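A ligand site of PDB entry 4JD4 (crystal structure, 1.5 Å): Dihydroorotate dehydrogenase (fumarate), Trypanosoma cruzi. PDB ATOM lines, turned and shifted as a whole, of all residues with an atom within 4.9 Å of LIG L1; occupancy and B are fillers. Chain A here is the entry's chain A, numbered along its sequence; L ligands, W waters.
The side-chain hydroxyl of Ser 196 lies within hydrogen-bond range of an oxygen (O3) of LG2 L2. The side-chain sulfur of Cys 249 sits at hydrogen-bond distance from an oxygen (O4) of LIG L1 (3.5 Å). O2 of LG2 L2 lies within hydrogen-bond range of N of Met 70, 3.1 Å away. The backbone NH of Gly 272 is in hydrogen-bond range of an oxygen (O9) of LIG L1 (2.9 Å). The side-chain amide nitrogen (ND2) of Asn 128 is in hydrogen-bond range of an oxygen (O4) of LG2 L2 (3.0 Å). OD1 of Asn 68 is in hydrogen-bond range of N1 of LG2 L2 (2.9 Å). The side-chain amino group (NZ) of Lys 44 is in hydrogen-bond range of an oxygen (O2) of LIG L1 (2.8 Å). NZ of Lys 165 sits at hydrogen-bond distance from O3 of LIG L1 (2.9 Å). The backbone carbonyl oxygen of Val 194 sits at hydrogen-bond distance from an oxygen (O4) of LIG L1 (2.8 Å). N2 of LIG L1 sits at hydrogen-bond distance from OG of Ser 45 (2.8 Å). The backbone NH (N) of Thr 273 sits at hydrogen-bond distance from an oxygen (O8) of LIG L1 (2.8 Å). The side-chain amide nitrogen (ND2) of Asn 128 lies within hydrogen-bond range of an oxygen (O1) of LIG L1 (3.4 Å). The backbone NH (N) of Leu 72 is in hydrogen-bond range of an oxygen (O1) of LG2 L2 (3.0 Å). N of Gly 223 is in hydrogen-bond range of O7 of LIG L1, 2.7 Å away. OD1 of Asn 195 is in hydrogen-bond range of N2 of LG2 L2. O3 of LIG L1 lies within hydrogen-bond range of O of Ala 20, 2.8 Å away. The backbone NH (N) of Gly 251 is in hydrogen-bond range of an oxygen (O7) of LIG L1 (2.8 Å). NZ of Lys 44 lies within salt-bridge range of O1 of LG2 L2. O8 of LIG L1 sits at hydrogen-bond distance from OG1 of Thr 273 (2.7 Å).
Ala 19 touches LIG L1 (CB to O3, 3.2 Å). CA of Gly 21 touches N3 of LIG L1 (3.3 Å). Tyr 59 touches LIG L1. Asn 68 touches LIG L1. Met 70 touches LIG L1. Leu 72 touches LIG L1 (CD1 to O2, 3.99 Å). Asn 195 touches LIG L1 (CA to O4, 3.3 Å). N of Ser 196 touches O4 of LIG L1, 3.8 Å away. Gly 222 touches LIG L1 (C to O7, 3.7 Å). Ile 226 touches LIG L1. Gly 250 touches LIG L1 (CA to O7, 3.4 Å). Hydrophobic or aromatic side chains that line LIG L1: Ala 19, Ala 20, Tyr 59, Met 70, Leu 72 and Ile 226. Within 4 Å of LIG L1: Ala 19, Ala 20, Gly 21, Lys 44, Ser 45, Tyr 59, Asn 68, Met 70, Leu 72, Asn 128, Lys 165, Val 194, Asn 195, Ser 196, Gly 222, Gly 223, Ile 226, Cys 249, Gly 250, Gly 251, Gly 272 and Thr 273. The nearest printed residue that does not touch LIG L1 is Val 271 (4.02 Å).
Water W2 bridges O5 of LIG L1 and N of Gly 222. Water W4 lies within hydrogen-bond range of an oxygen (O9) of LIG L1 (2.8 Å), the backbone NH (N) of Ala 274 (2.8 Å) and the backbone carbonyl oxygen (O) of Val 252 (3.0 Å). Water W3 lies within hydrogen-bond range of the side-chain hydroxyl (OG) of Ser 98 (2.6 Å), the side-chain carboxylate (OE1) of Glu 126 (2.7 Å) and an oxygen (O1) of LIG L1 (2.9 Å). Water W1 lies within hydrogen-bond range of NZ of Lys 44 (3.0 Å) and O of Gly 21 (3.0 Å).
N of Ser 66 sits at hydrogen-bond distance from O of Gly 222, at 3.0 Å. SG of Cys 249 lies within hydrogen-bond range of OE1 of Gln 270. The side-chain amide oxygen of Asn 68 is in hydrogen-bond range of the backbone NH of Met 70 (3.4 Å). The side-chain hydroxyl (OG) of Ser 45 lies within hydrogen-bond range of the side-chain hydroxyl (OG) of Ser 98, at 2.6 Å. The backbone NH (N) of Val 194 is in hydrogen-bond range of the backbone carbonyl oxygen (O) of Cys 249. OD1 of Asn 195 is in hydrogen-bond range of OG of Ser 196, 3.5 Å away. The side-chain hydroxyl (OG) of Ser 45 is in hydrogen-bond range of the side-chain amide nitrogen (ND2) of Asn 128 (3.3 Å). N of Ala 19 is in hydrogen-bond range of O of Val 271.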
ATOM      1  N   ALA A  19     -14.027  16.228  22.106  1.00  0.00           N
ATOM      2  CA  ALA A  19     -14.054  17.560  21.574  1.00  0.00           C
ATOM      3  C   ALA A  19     -14.468  17.575  20.104  1.00  0.00           C
ATOM      4  O   ALA A  19     -14.036  16.708  19.328  1.00  0.00           O
ATOM      5  CB  ALA A  19     -12.715  18.224  21.717  1.00  0.00           C
ATOM      6  N   ALA A  20     -15.283  18.506  19.664  1.00  0.00           N
ATOM      7  CA  ALA A  20     -15.645  18.556  18.248  1.00  0.00           C
ATOM      8  C   ALA A  20     -14.423  18.584  17.421  1.00  0.00           C
ATOM      9  O   ALA A  20     -13.408  19.240  17.689  1.00  0.00           O
ATOM     10  CB  ALA A  20     -16.542  19.769  17.969  1.00  0.00           C
ATOM     11  N   GLY A  21     -14.480  17.874  16.322  1.00  0.00           N
ATOM     12  CA  GLY A  21     -13.378  17.718  15.400  1.00  0.00           C
ATOM     13  C   GLY A  21     -12.540  16.479  15.531  1.00  0.00           C
ATOM     14  O   GLY A  21     -11.857  16.080  14.596  1.00  0.00           O
ATOM     15  N   VAL A  22     -12.482  15.922  16.759  1.00  0.00           N
ATOM     16  CA  VAL A  22     -11.662  14.718  17.010  1.00  0.00           C
ATOM     17  C   VAL A  22     -12.583  13.467  17.080  1.00  0.00           C
ATOM     18  O   VAL A  22     -13.578  13.432  17.792  1.00  0.00           O
ATOM     19  CB  VAL A  22     -10.871  14.901  18.364  1.00  0.00           C
ATOM     20  CG1 VAL A  22     -10.096  13.650  18.679  1.00  0.00           C
ATOM     21  CG2 VAL A  22     -10.012  16.140  18.252  1.00  0.00           C
ATOM     22  N   LYS A  44     -18.427  16.357  14.079  1.00  0.00           N
ATOM     23  CA  LYS A  44     -17.509  17.335  13.516  1.00  0.00           C
ATOM     24  C   LYS A  44     -18.324  18.572  13.146  1.00  0.00           C
ATOM     25  O   LYS A  44     -19.384  18.443  12.478  1.00  0.00           O
ATOM     26  CB  LYS A  44     -16.859  16.744  12.242  1.00  0.00           C
ATOM     27  CG  LYS A  44     -16.118  17.706  11.359  1.00  0.00           C
ATOM     28  CD  LYS A  44     -14.794  18.245  11.930  1.00  0.00           C
ATOM     29  CE  LYS A  44     -14.138  19.440  11.222  1.00  0.00           C
ATOM     30  NZ  LYS A  44     -12.902  20.030  11.948  1.00  0.00           N
ATOM     31  N   SER A  45     -17.808  19.752  13.390  1.00  0.00           N
ATOM     32  CA  SER A  45     -18.498  21.007  12.961  1.00  0.00           C
ATOM     33  C   SER A  45     -18.652  20.920  11.442  1.00  0.00           C
ATOM     34  O   SER A  45     -17.724  20.637  10.687  1.00  0.00           O
ATOM     35  CB  SER A  45     -17.730  22.251  13.220  1.00  0.00           C
ATOM     36  OG  SER A  45     -17.606  22.479  14.659  1.00  0.00           O
ATOM     37  N   TYR A  59      -2.415  18.594  10.766  1.00  0.00           N
ATOM     38  CA  TYR A  59      -2.371  18.367  12.178  1.00  0.00           C
ATOM     39  C   TYR A  59      -1.063  17.736  12.536  1.00  0.00           C
ATOM     40  O   TYR A  59      -0.608  16.827  11.903  1.00  0.00           O
ATOM     41  CB  TYR A  59      -3.518  17.383  12.570  1.00  0.00           C
ATOM     42  CG  TYR A  59      -3.458  16.846  14.002  1.00  0.00           C
ATOM     43  CD1 TYR A  59      -4.054  17.549  15.065  1.00  0.00           C
ATOM     44  CD2 TYR A  59      -2.823  15.692  14.297  1.00  0.00           C
ATOM     45  CE1 TYR A  59      -4.002  17.096  16.331  1.00  0.00           C
ATOM     46  CE2 TYR A  59      -2.763  15.237  15.608  1.00  0.00           C
ATOM     47  CZ  TYR A  59      -3.337  15.948  16.618  1.00  0.00           C
ATOM     48  OH  TYR A  59      -3.283  15.468  17.910  1.00  0.00           O
ATOM     49  N   SER A  66      -0.792  19.900  20.508  1.00  0.00           N
ATOM     50  CA  SER A  66      -1.009  19.779  19.083  1.00  0.00           C
ATOM     51  C   SER A  66      -1.200  21.136  18.434  1.00  0.00           C
ATOM     52  O   SER A  66      -1.526  22.143  19.069  1.00  0.00           O
ATOM     53  CB  SER A  66      -2.211  18.884  18.803  1.00  0.00           C
ATOM     54  OG  SER A  66      -3.437  19.550  19.208  1.00  0.00           O
ATOM     55  N   ASN A  68      -3.112  22.587  14.657  1.00  0.00           N
ATOM     56  CA  ASN A  68      -3.932  22.204  13.512  1.00  0.00           C
ATOM     57  C   ASN A  68      -4.454  23.397  12.787  1.00  0.00           C
ATOM     58  O   ASN A  68      -4.825  24.412  13.298  1.00  0.00           O
ATOM     59  CB  ASN A  68      -5.103  21.279  13.899  1.00  0.00           C
ATOM     60  CG  ASN A  68      -6.334  22.029  14.262  1.00  0.00           C
ATOM     61  OD1 ASN A  68      -7.163  22.448  13.408  1.00  0.00           O
ATOM     62  ND2 ASN A  68      -6.543  22.198  15.560  1.00  0.00           N
ATOM     63  N   MET A  70      -7.001  22.494  10.038  1.00  0.00           N
ATOM     64  CA  MET A  70      -7.658  21.426   9.267  1.00  0.00           C
ATOM     65  C   MET A  70      -8.402  22.046   8.107  1.00  0.00           C
ATOM     66  O   MET A  70      -8.475  21.393   7.048  1.00  0.00           O
ATOM     67  CB  MET A  70      -8.592  20.614  10.132  1.00  0.00           C
ATOM     68  CG  MET A  70      -8.063  19.927  11.332  1.00  0.00           C
ATOM     69  SD  MET A  70      -6.778  18.739  10.995  1.00  0.00           S
ATOM     70  CE  MET A  70      -7.627  17.431  10.315  1.00  0.00           C
ATOM     71  N   LEU A  72     -11.707  22.810   8.277  1.00  0.00           N
ATOM     72  CA  LEU A  72     -13.074  22.296   8.389  1.00  0.00           C
ATOM     73  C   LEU A  72     -13.413  21.223   7.376  1.00  0.00           C
ATOM     74  O   LEU A  72     -14.494  21.302   6.740  1.00  0.00           O
ATOM     75  CB  LEU A  72     -14.135  23.412   8.462  1.00  0.00           C
ATOM     76  CG  LEU A  72     -15.405  22.886   9.133  1.00  0.00           C
ATOM     77  CD1 LEU A  72     -15.355  23.098  10.636  1.00  0.00           C
ATOM     78  CD2 LEU A  72     -16.657  23.522   8.652  1.00  0.00           C
ATOM     79  N   SER A  98     -22.442  19.647  15.965  1.00  0.00           N
ATOM     80  CA  SER A  98     -21.794  20.945  15.872  1.00  0.00           C
ATOM     81  C   SER A  98     -21.967  21.486  14.497  1.00  0.00           C
ATOM     82  O   SER A  98     -21.796  20.783  13.478  1.00  0.00           O
ATOM     83  CB  SER A  98     -20.314  20.828  16.261  1.00  0.00           C
ATOM     84  OG  SER A  98     -19.737  22.098  16.136  1.00  0.00           O
ATOM     85  N   GLU A 126     -24.509  22.318  19.205  1.00  0.00           N
ATOM     86  CA  GLU A 126     -23.363  23.138  19.599  1.00  0.00           C
ATOM     87  C   GLU A 126     -22.987  24.009  18.460  1.00  0.00           C
ATOM     88  O   GLU A 126     -22.560  23.537  17.402  1.00  0.00           O
ATOM     89  CB  GLU A 126     -22.204  22.261  20.080  1.00  0.00           C
ATOM     90  CG  GLU A 126     -21.014  23.063  20.669  1.00  0.00           C
ATOM     91  CD  GLU A 126     -19.822  22.159  21.250  1.00  0.00           C
ATOM     92  OE1 GLU A 126     -18.919  21.761  20.455  1.00  0.00           O
ATOM     93  OE2 GLU A 126     -19.746  21.864  22.500  1.00  0.00           O
ATOM     94  N   ASN A 128     -20.532  26.481  16.717  1.00  0.00           N
ATOM     95  CA  ASN A 128     -19.110  26.855  16.773  1.00  0.00           C
ATOM     96  C   ASN A 128     -18.913  28.253  16.279  1.00  0.00           C
ATOM     97  O   ASN A 128     -19.031  28.518  15.062  1.00  0.00           O
ATOM     98  CB  ASN A 128     -18.293  25.865  15.953  1.00  0.00           C
ATOM     99  CG  ASN A 128     -16.828  26.188  15.870  1.00  0.00           C
ATOM    100  OD1 ASN A 128     -16.372  27.104  16.450  1.00  0.00           O
ATOM    101  ND2 ASN A 128     -16.092  25.354  15.128  1.00  0.00           N
ATOM    102  N   LYS A 165     -19.795  27.019  21.256  1.00  0.00           N
ATOM    103  CA  LYS A 165     -18.395  26.750  21.428  1.00  0.00           C
ATOM    104  C   LYS A 165     -17.651  28.069  21.210  1.00  0.00           C
ATOM    105  O   LYS A 165     -17.745  28.682  20.150  1.00  0.00           O
ATOM    106  CB  LYS A 165     -17.975  25.711  20.447  1.00  0.00           C
ATOM    107  CG  LYS A 165     -16.514  25.304  20.399  1.00  0.00           C
ATOM    108  CD  LYS A 165     -16.120  24.463  21.537  1.00  0.00           C
ATOM    109  CE  LYS A 165     -14.708  23.858  21.450  1.00  0.00           C
ATOM    110  NZ  LYS A 165     -14.653  22.801  20.458  1.00  0.00           N
ATOM    111  N   VAL A 194     -12.756  25.641  25.940  1.00  0.00           N
ATOM    112  CA  VAL A 194     -12.463  26.520  24.819  1.00  0.00           C
ATOM    113  C   VAL A 194     -12.135  25.733  23.562  1.00  0.00           C
ATOM    114  O   VAL A 194     -11.719  24.555  23.626  1.00  0.00           O
ATOM    115  CB  VAL A 194     -11.286  27.465  25.167  1.00  0.00           C
ATOM    116  CG1 VAL A 194     -11.623  28.432  26.298  1.00  0.00           C
ATOM    117  CG2 VAL A 194     -10.011  26.674  25.487  1.00  0.00           C
ATOM    118  N   ASN A 195     -12.300  26.456  22.455  1.00  0.00           N
ATOM    119  CA  ASN A 195     -11.654  26.091  21.190  1.00  0.00           C
ATOM    120  C   ASN A 195     -10.137  26.225  21.288  1.00  0.00           C
ATOM    121  O   ASN A 195      -9.599  26.684  22.307  1.00  0.00           O
ATOM    122  CB  ASN A 195     -12.306  26.909  20.052  1.00  0.00           C
ATOM    123  CG  ASN A 195     -12.392  26.111  18.764  1.00  0.00           C
ATOM    124  OD1 ASN A 195     -11.407  25.472  18.354  1.00  0.00           O
ATOM    125  ND2 ASN A 195     -13.523  26.169  18.100  1.00  0.00           N
ATOM    126  N   SER A 196      -9.398  25.787  20.286  1.00  0.00           N
ATOM    127  CA  SER A 196      -7.972  25.911  20.242  1.00  0.00           C
ATOM    128  C   SER A 196      -7.538  27.368  20.413  1.00  0.00           C
ATOM    129  O   SER A 196      -8.239  28.381  20.120  1.00  0.00           O
ATOM    130  CB  SER A 196      -7.470  25.233  18.964  1.00  0.00           C
ATOM    131  OG  SER A 196      -7.985  25.845  17.812  1.00  0.00           O
ATOM    132  N   GLY A 222      -3.721  22.991  20.886  1.00  0.00           N
ATOM    133  CA  GLY A 222      -4.472  22.246  21.896  1.00  0.00           C
ATOM    134  C   GLY A 222      -3.470  21.505  22.802  1.00  0.00           C
ATOM    135  O   GLY A 222      -2.264  21.465  22.543  1.00  0.00           O
ATOM    136  N   GLY A 223      -4.015  20.845  23.833  1.00  0.00           N
ATOM    137  CA  GLY A 223      -3.230  20.034  24.713  1.00  0.00           C
ATOM    138  C   GLY A 223      -2.647  20.731  25.932  1.00  0.00           C
ATOM    139  O   GLY A 223      -3.262  21.646  26.458  1.00  0.00           O
ATOM    140  N   ILE A 226      -2.436  24.570  26.742  1.00  0.00           N
ATOM    141  CA  ILE A 226      -3.642  25.389  26.908  1.00  0.00           C
ATOM    142  C   ILE A 226      -4.481  25.171  28.168  1.00  0.00           C
ATOM    143  O   ILE A 226      -5.455  25.889  28.367  1.00  0.00           O
ATOM    144  CB  ILE A 226      -4.514  25.399  25.658  1.00  0.00           C
ATOM    145  CG1 ILE A 226      -5.461  24.179  25.591  1.00  0.00           C
ATOM    146  CG2 ILE A 226      -3.703  25.557  24.364  1.00  0.00           C
ATOM    147  CD1 ILE A 226      -6.611  24.349  24.600  1.00  0.00           C
ATOM    148  N   CYS A 249     -13.259  22.312  27.915  1.00  0.00           N
ATOM    149  CA  CYS A 249     -12.456  21.696  26.906  1.00  0.00           C
ATOM    150  C   CYS A 249     -11.089  22.374  26.902  1.00  0.00           C
ATOM    151  O   CYS A 249     -11.004  23.591  26.878  1.00  0.00           O
ATOM    152  CB  CYS A 249     -13.147  21.932  25.550  1.00  0.00           C
ATOM    153  SG  CYS A 249     -12.359  20.965  24.202  1.00  0.00           S
ATOM    154  N   GLY A 250     -10.033  21.609  26.920  1.00  0.00           N
ATOM    155  CA  GLY A 250      -8.681  22.123  26.743  1.00  0.00           C
ATOM    156  C   GLY A 250      -7.718  21.500  27.718  1.00  0.00           C
ATOM    157  O   GLY A 250      -7.891  21.611  28.939  1.00  0.00           O
ATOM    158  N   GLY A 251      -6.757  20.753  27.220  1.00  0.00           N
ATOM    159  CA  GLY A 251      -5.677  20.259  28.069  1.00  0.00           C
ATOM    160  C   GLY A 251      -6.019  19.098  28.922  1.00  0.00           C
ATOM    161  O   GLY A 251      -5.242  18.805  29.854  1.00  0.00           O
ATOM    162  N   VAL A 252      -7.121  18.373  28.645  1.00  0.00           N
ATOM    163  CA  VAL A 252      -7.469  17.220  29.495  1.00  0.00           C
ATOM    164  C   VAL A 252      -6.667  15.979  29.021  1.00  0.00           C
ATOM    165  O   VAL A 252      -6.935  15.464  27.951  1.00  0.00           O
ATOM    166  CB  VAL A 252      -8.947  16.944  29.556  1.00  0.00           C
ATOM    167  CG1 VAL A 252      -9.212  15.673  30.354  1.00  0.00           C
ATOM    168  CG2 VAL A 252      -9.689  18.146  30.177  1.00  0.00           C
ATOM    169  N   GLN A 270     -14.694  17.817  27.791  1.00  0.00           N
ATOM    170  CA  GLN A 270     -14.379  17.394  26.451  1.00  0.00           C
ATOM    171  C   GLN A 270     -12.906  17.129  26.307  1.00  0.00           C
ATOM    172  O   GLN A 270     -12.071  17.818  26.920  1.00  0.00           O
ATOM    173  CB  GLN A 270     -14.841  18.356  25.407  1.00  0.00           C
ATOM    174  CG  GLN A 270     -16.273  18.950  25.604  1.00  0.00           C
ATOM    175  CD  GLN A 270     -16.734  19.716  24.468  1.00  0.00           C
ATOM    176  OE1 GLN A 270     -15.968  20.325  23.740  1.00  0.00           O
ATOM    177  NE2 GLN A 270     -18.038  19.720  24.249  1.00  0.00           N
ATOM    178  N   VAL A 271     -12.572  16.151  25.441  1.00  0.00           N
ATOM    179  CA  VAL A 271     -11.162  15.724  25.275  1.00  0.00           C
ATOM    180  C   VAL A 271     -10.825  15.740  23.776  1.00  0.00           C
ATOM    181  O   VAL A 271     -11.482  15.024  22.994  1.00  0.00           O
ATOM    182  CB  VAL A 271     -11.023  14.300  25.828  1.00  0.00           C
ATOM    183  CG1 VAL A 271      -9.585  13.889  25.808  1.00  0.00           C
ATOM    184  CG2 VAL A 271     -11.604  14.191  27.294  1.00  0.00           C
ATOM    185  N   GLY A 272      -9.842  16.560  23.353  1.00  0.00           N
ATOM    186  CA  GLY A 272      -9.446  16.740  22.011  1.00  0.00           C
ATOM    187  C   GLY A 272      -8.159  16.046  21.714  1.00  0.00           C
ATOM    188  O   GLY A 272      -8.062  14.834  21.418  1.00  0.00           O
ATOM    189  N   THR A 273      -7.061  16.803  21.852  1.00  0.00           N
ATOM    190  CA  THR A 273      -5.731  16.319  21.567  1.00  0.00           C
ATOM    191  C   THR A 273      -5.435  15.016  22.219  1.00  0.00           C
ATOM    192  O   THR A 273      -4.872  14.075  21.565  1.00  0.00           O
ATOM    193  CB  THR A 273      -4.684  17.389  21.980  1.00  0.00           C
ATOM    194  OG1 THR A 273      -4.884  18.604  21.259  1.00  0.00           O
ATOM    195  CG2 THR A 273      -3.235  16.877  21.762  1.00  0.00           C
ATOM    196  N   ALA A 274      -5.716  14.837  23.512  1.00  0.00           N
ATOM    197  CA  ALA A 274      -5.362  13.540  24.165  1.00  0.00           C
ATOM    198  C   ALA A 274      -6.106  12.343  23.596  1.00  0.00           C
ATOM    199  O   ALA A 274      -5.582  11.245  23.559  1.00  0.00           O
ATOM    200  CB  ALA A 274      -5.628  13.623  25.649  1.00  0.00           C
HETATM  201  N1  LIG L   1     -13.441  22.572  17.468  1.00  0.00           N
HETATM  202  C1  LIG L   1     -14.685  22.761  16.977  1.00  0.00           C
HETATM  203  O1  LIG L   1     -15.532  23.297  17.716  1.00  0.00           O
HETATM  204  N2  LIG L   1     -15.045  22.196  15.797  1.00  0.00           N
HETATM  205  C2  LIG L   1     -14.216  21.545  15.006  1.00  0.00           C
HETATM  206  O2  LIG L   1     -14.581  21.014  13.945  1.00  0.00           O
HETATM  207  C3  LIG L   1     -12.864  21.324  15.476  1.00  0.00           C
HETATM  208  N3  LIG L   1     -11.955  20.633  14.729  1.00  0.00           N
HETATM  209  C4  LIG L   1     -10.820  20.251  15.367  1.00  0.00           C
HETATM  210  C5  LIG L   1      -9.966  19.386  14.716  1.00  0.00           C
HETATM  211  C6  LIG L   1      -8.789  18.976  15.272  1.00  0.00           C
HETATM  212  C7  LIG L   1      -7.813  18.043  14.584  1.00  0.00           C
HETATM  213  C8  LIG L   1      -8.375  19.438  16.554  1.00  0.00           C
HETATM  214  C9  LIG L   1      -7.093  19.093  17.267  1.00  0.00           C
HETATM  215  C10 LIG L   1      -9.233  20.316  17.210  1.00  0.00           C
HETATM  216  C11 LIG L   1     -10.444  20.739  16.652  1.00  0.00           C
HETATM  217  N4  LIG L   1     -11.296  21.612  17.287  1.00  0.00           N
HETATM  218  C12 LIG L   1     -12.541  21.869  16.773  1.00  0.00           C
HETATM  219  C13 LIG L   1     -11.006  22.141  18.573  1.00  0.00           C
HETATM  220  C14 LIG L   1     -11.213  21.146  19.709  1.00  0.00           C
HETATM  221  O3  LIG L   1     -12.619  20.830  19.826  1.00  0.00           O
HETATM  222  C15 LIG L   1     -10.827  21.641  21.057  1.00  0.00           C
HETATM  223  O4  LIG L   1     -11.549  22.831  21.389  1.00  0.00           O
HETATM  224  C16 LIG L   1      -9.316  21.991  21.147  1.00  0.00           C
HETATM  225  O5  LIG L   1      -8.519  20.959  20.453  1.00  0.00           O
HETATM  226  C17 LIG L   1      -8.843  22.120  22.603  1.00  0.00           C
HETATM  227  O6  LIG L   1      -8.995  20.882  23.336  1.00  0.00           O
HETATM  228  P1  LIG L   1      -7.700  19.948  23.625  1.00  0.00           P
HETATM  229  O7  LIG L   1      -6.691  20.726  24.420  1.00  0.00           O
HETATM  230  O8  LIG L   1      -7.170  19.553  22.278  1.00  0.00           O
HETATM  231  O9  LIG L   1      -8.269  18.787  24.350  1.00  0.00           O
HETATM  232  O1  LG2 L   2     -11.246  22.471  11.208  1.00  0.00           O
HETATM  233  C1  LG2 L   2     -10.488  23.395  11.700  1.00  0.00           C
HETATM  234  O2  LG2 L   2      -9.376  23.926  11.330  1.00  0.00           O
HETATM  235  C2  LG2 L   2     -10.764  23.754  13.101  1.00  0.00           C
HETATM  236  N1  LG2 L   2      -9.741  23.603  14.053  1.00  0.00           N
HETATM  237  C3  LG2 L   2      -9.948  24.019  15.404  1.00  0.00           C
HETATM  238  O3  LG2 L   2      -8.959  23.790  16.197  1.00  0.00           O
HETATM  239  N2  LG2 L   2     -11.129  24.591  15.784  1.00  0.00           N
HETATM  240  C4  LG2 L   2     -12.144  24.813  14.862  1.00  0.00           C
HETATM  241  O4  LG2 L   2     -13.140  25.362  15.298  1.00  0.00           O
HETATM  242  C5  LG2 L   2     -11.916  24.464  13.507  1.00  0.00           C
HETATM  243  C6  LG2 L   2     -12.972  24.848  12.508  1.00  0.00           C
HETATM  244  C7  LG2 L   2     -12.889  26.404  12.220  1.00  0.00           C
HETATM  245  C8  LG2 L   2     -13.621  26.776  10.982  1.00  0.00           C
HETATM  246  C9  LG2 L   2     -15.010  26.998  11.092  1.00  0.00           C
HETATM  247  C10 LG2 L   2     -15.806  27.324   9.987  1.00  0.00           C
HETATM  248  C11 LG2 L   2     -15.189  27.306   8.752  1.00  0.00           C
HETATM  249  C12 LG2 L   2     -13.855  27.168   8.628  1.00  0.00           C
HETATM  250  C13 LG2 L   2     -13.015  26.846   9.725  1.00  0.00           C
HETATM  251  C14 LG2 L   2     -11.643  26.549   9.531  1.00  0.00           C
HETATM  252  O5  LG2 L   2     -10.814  27.630   9.537  1.00  0.00           O
HETATM  253  O   HOH W   1     -11.272  17.554  12.080  1.00  0.00           O
HETATM  254  O   HOH W   2      -6.622  22.455  19.193  1.00  0.00           O
HETATM  255  O   HOH W   3     -18.336  22.956  18.162  1.00  0.00           O
HETATM  256  O   HOH W   4      -6.587  16.818  25.323  1.00  0.00           O
HETATM  257  O   HOH W   5      -9.473  18.804  26.781  1.00  0.00           O
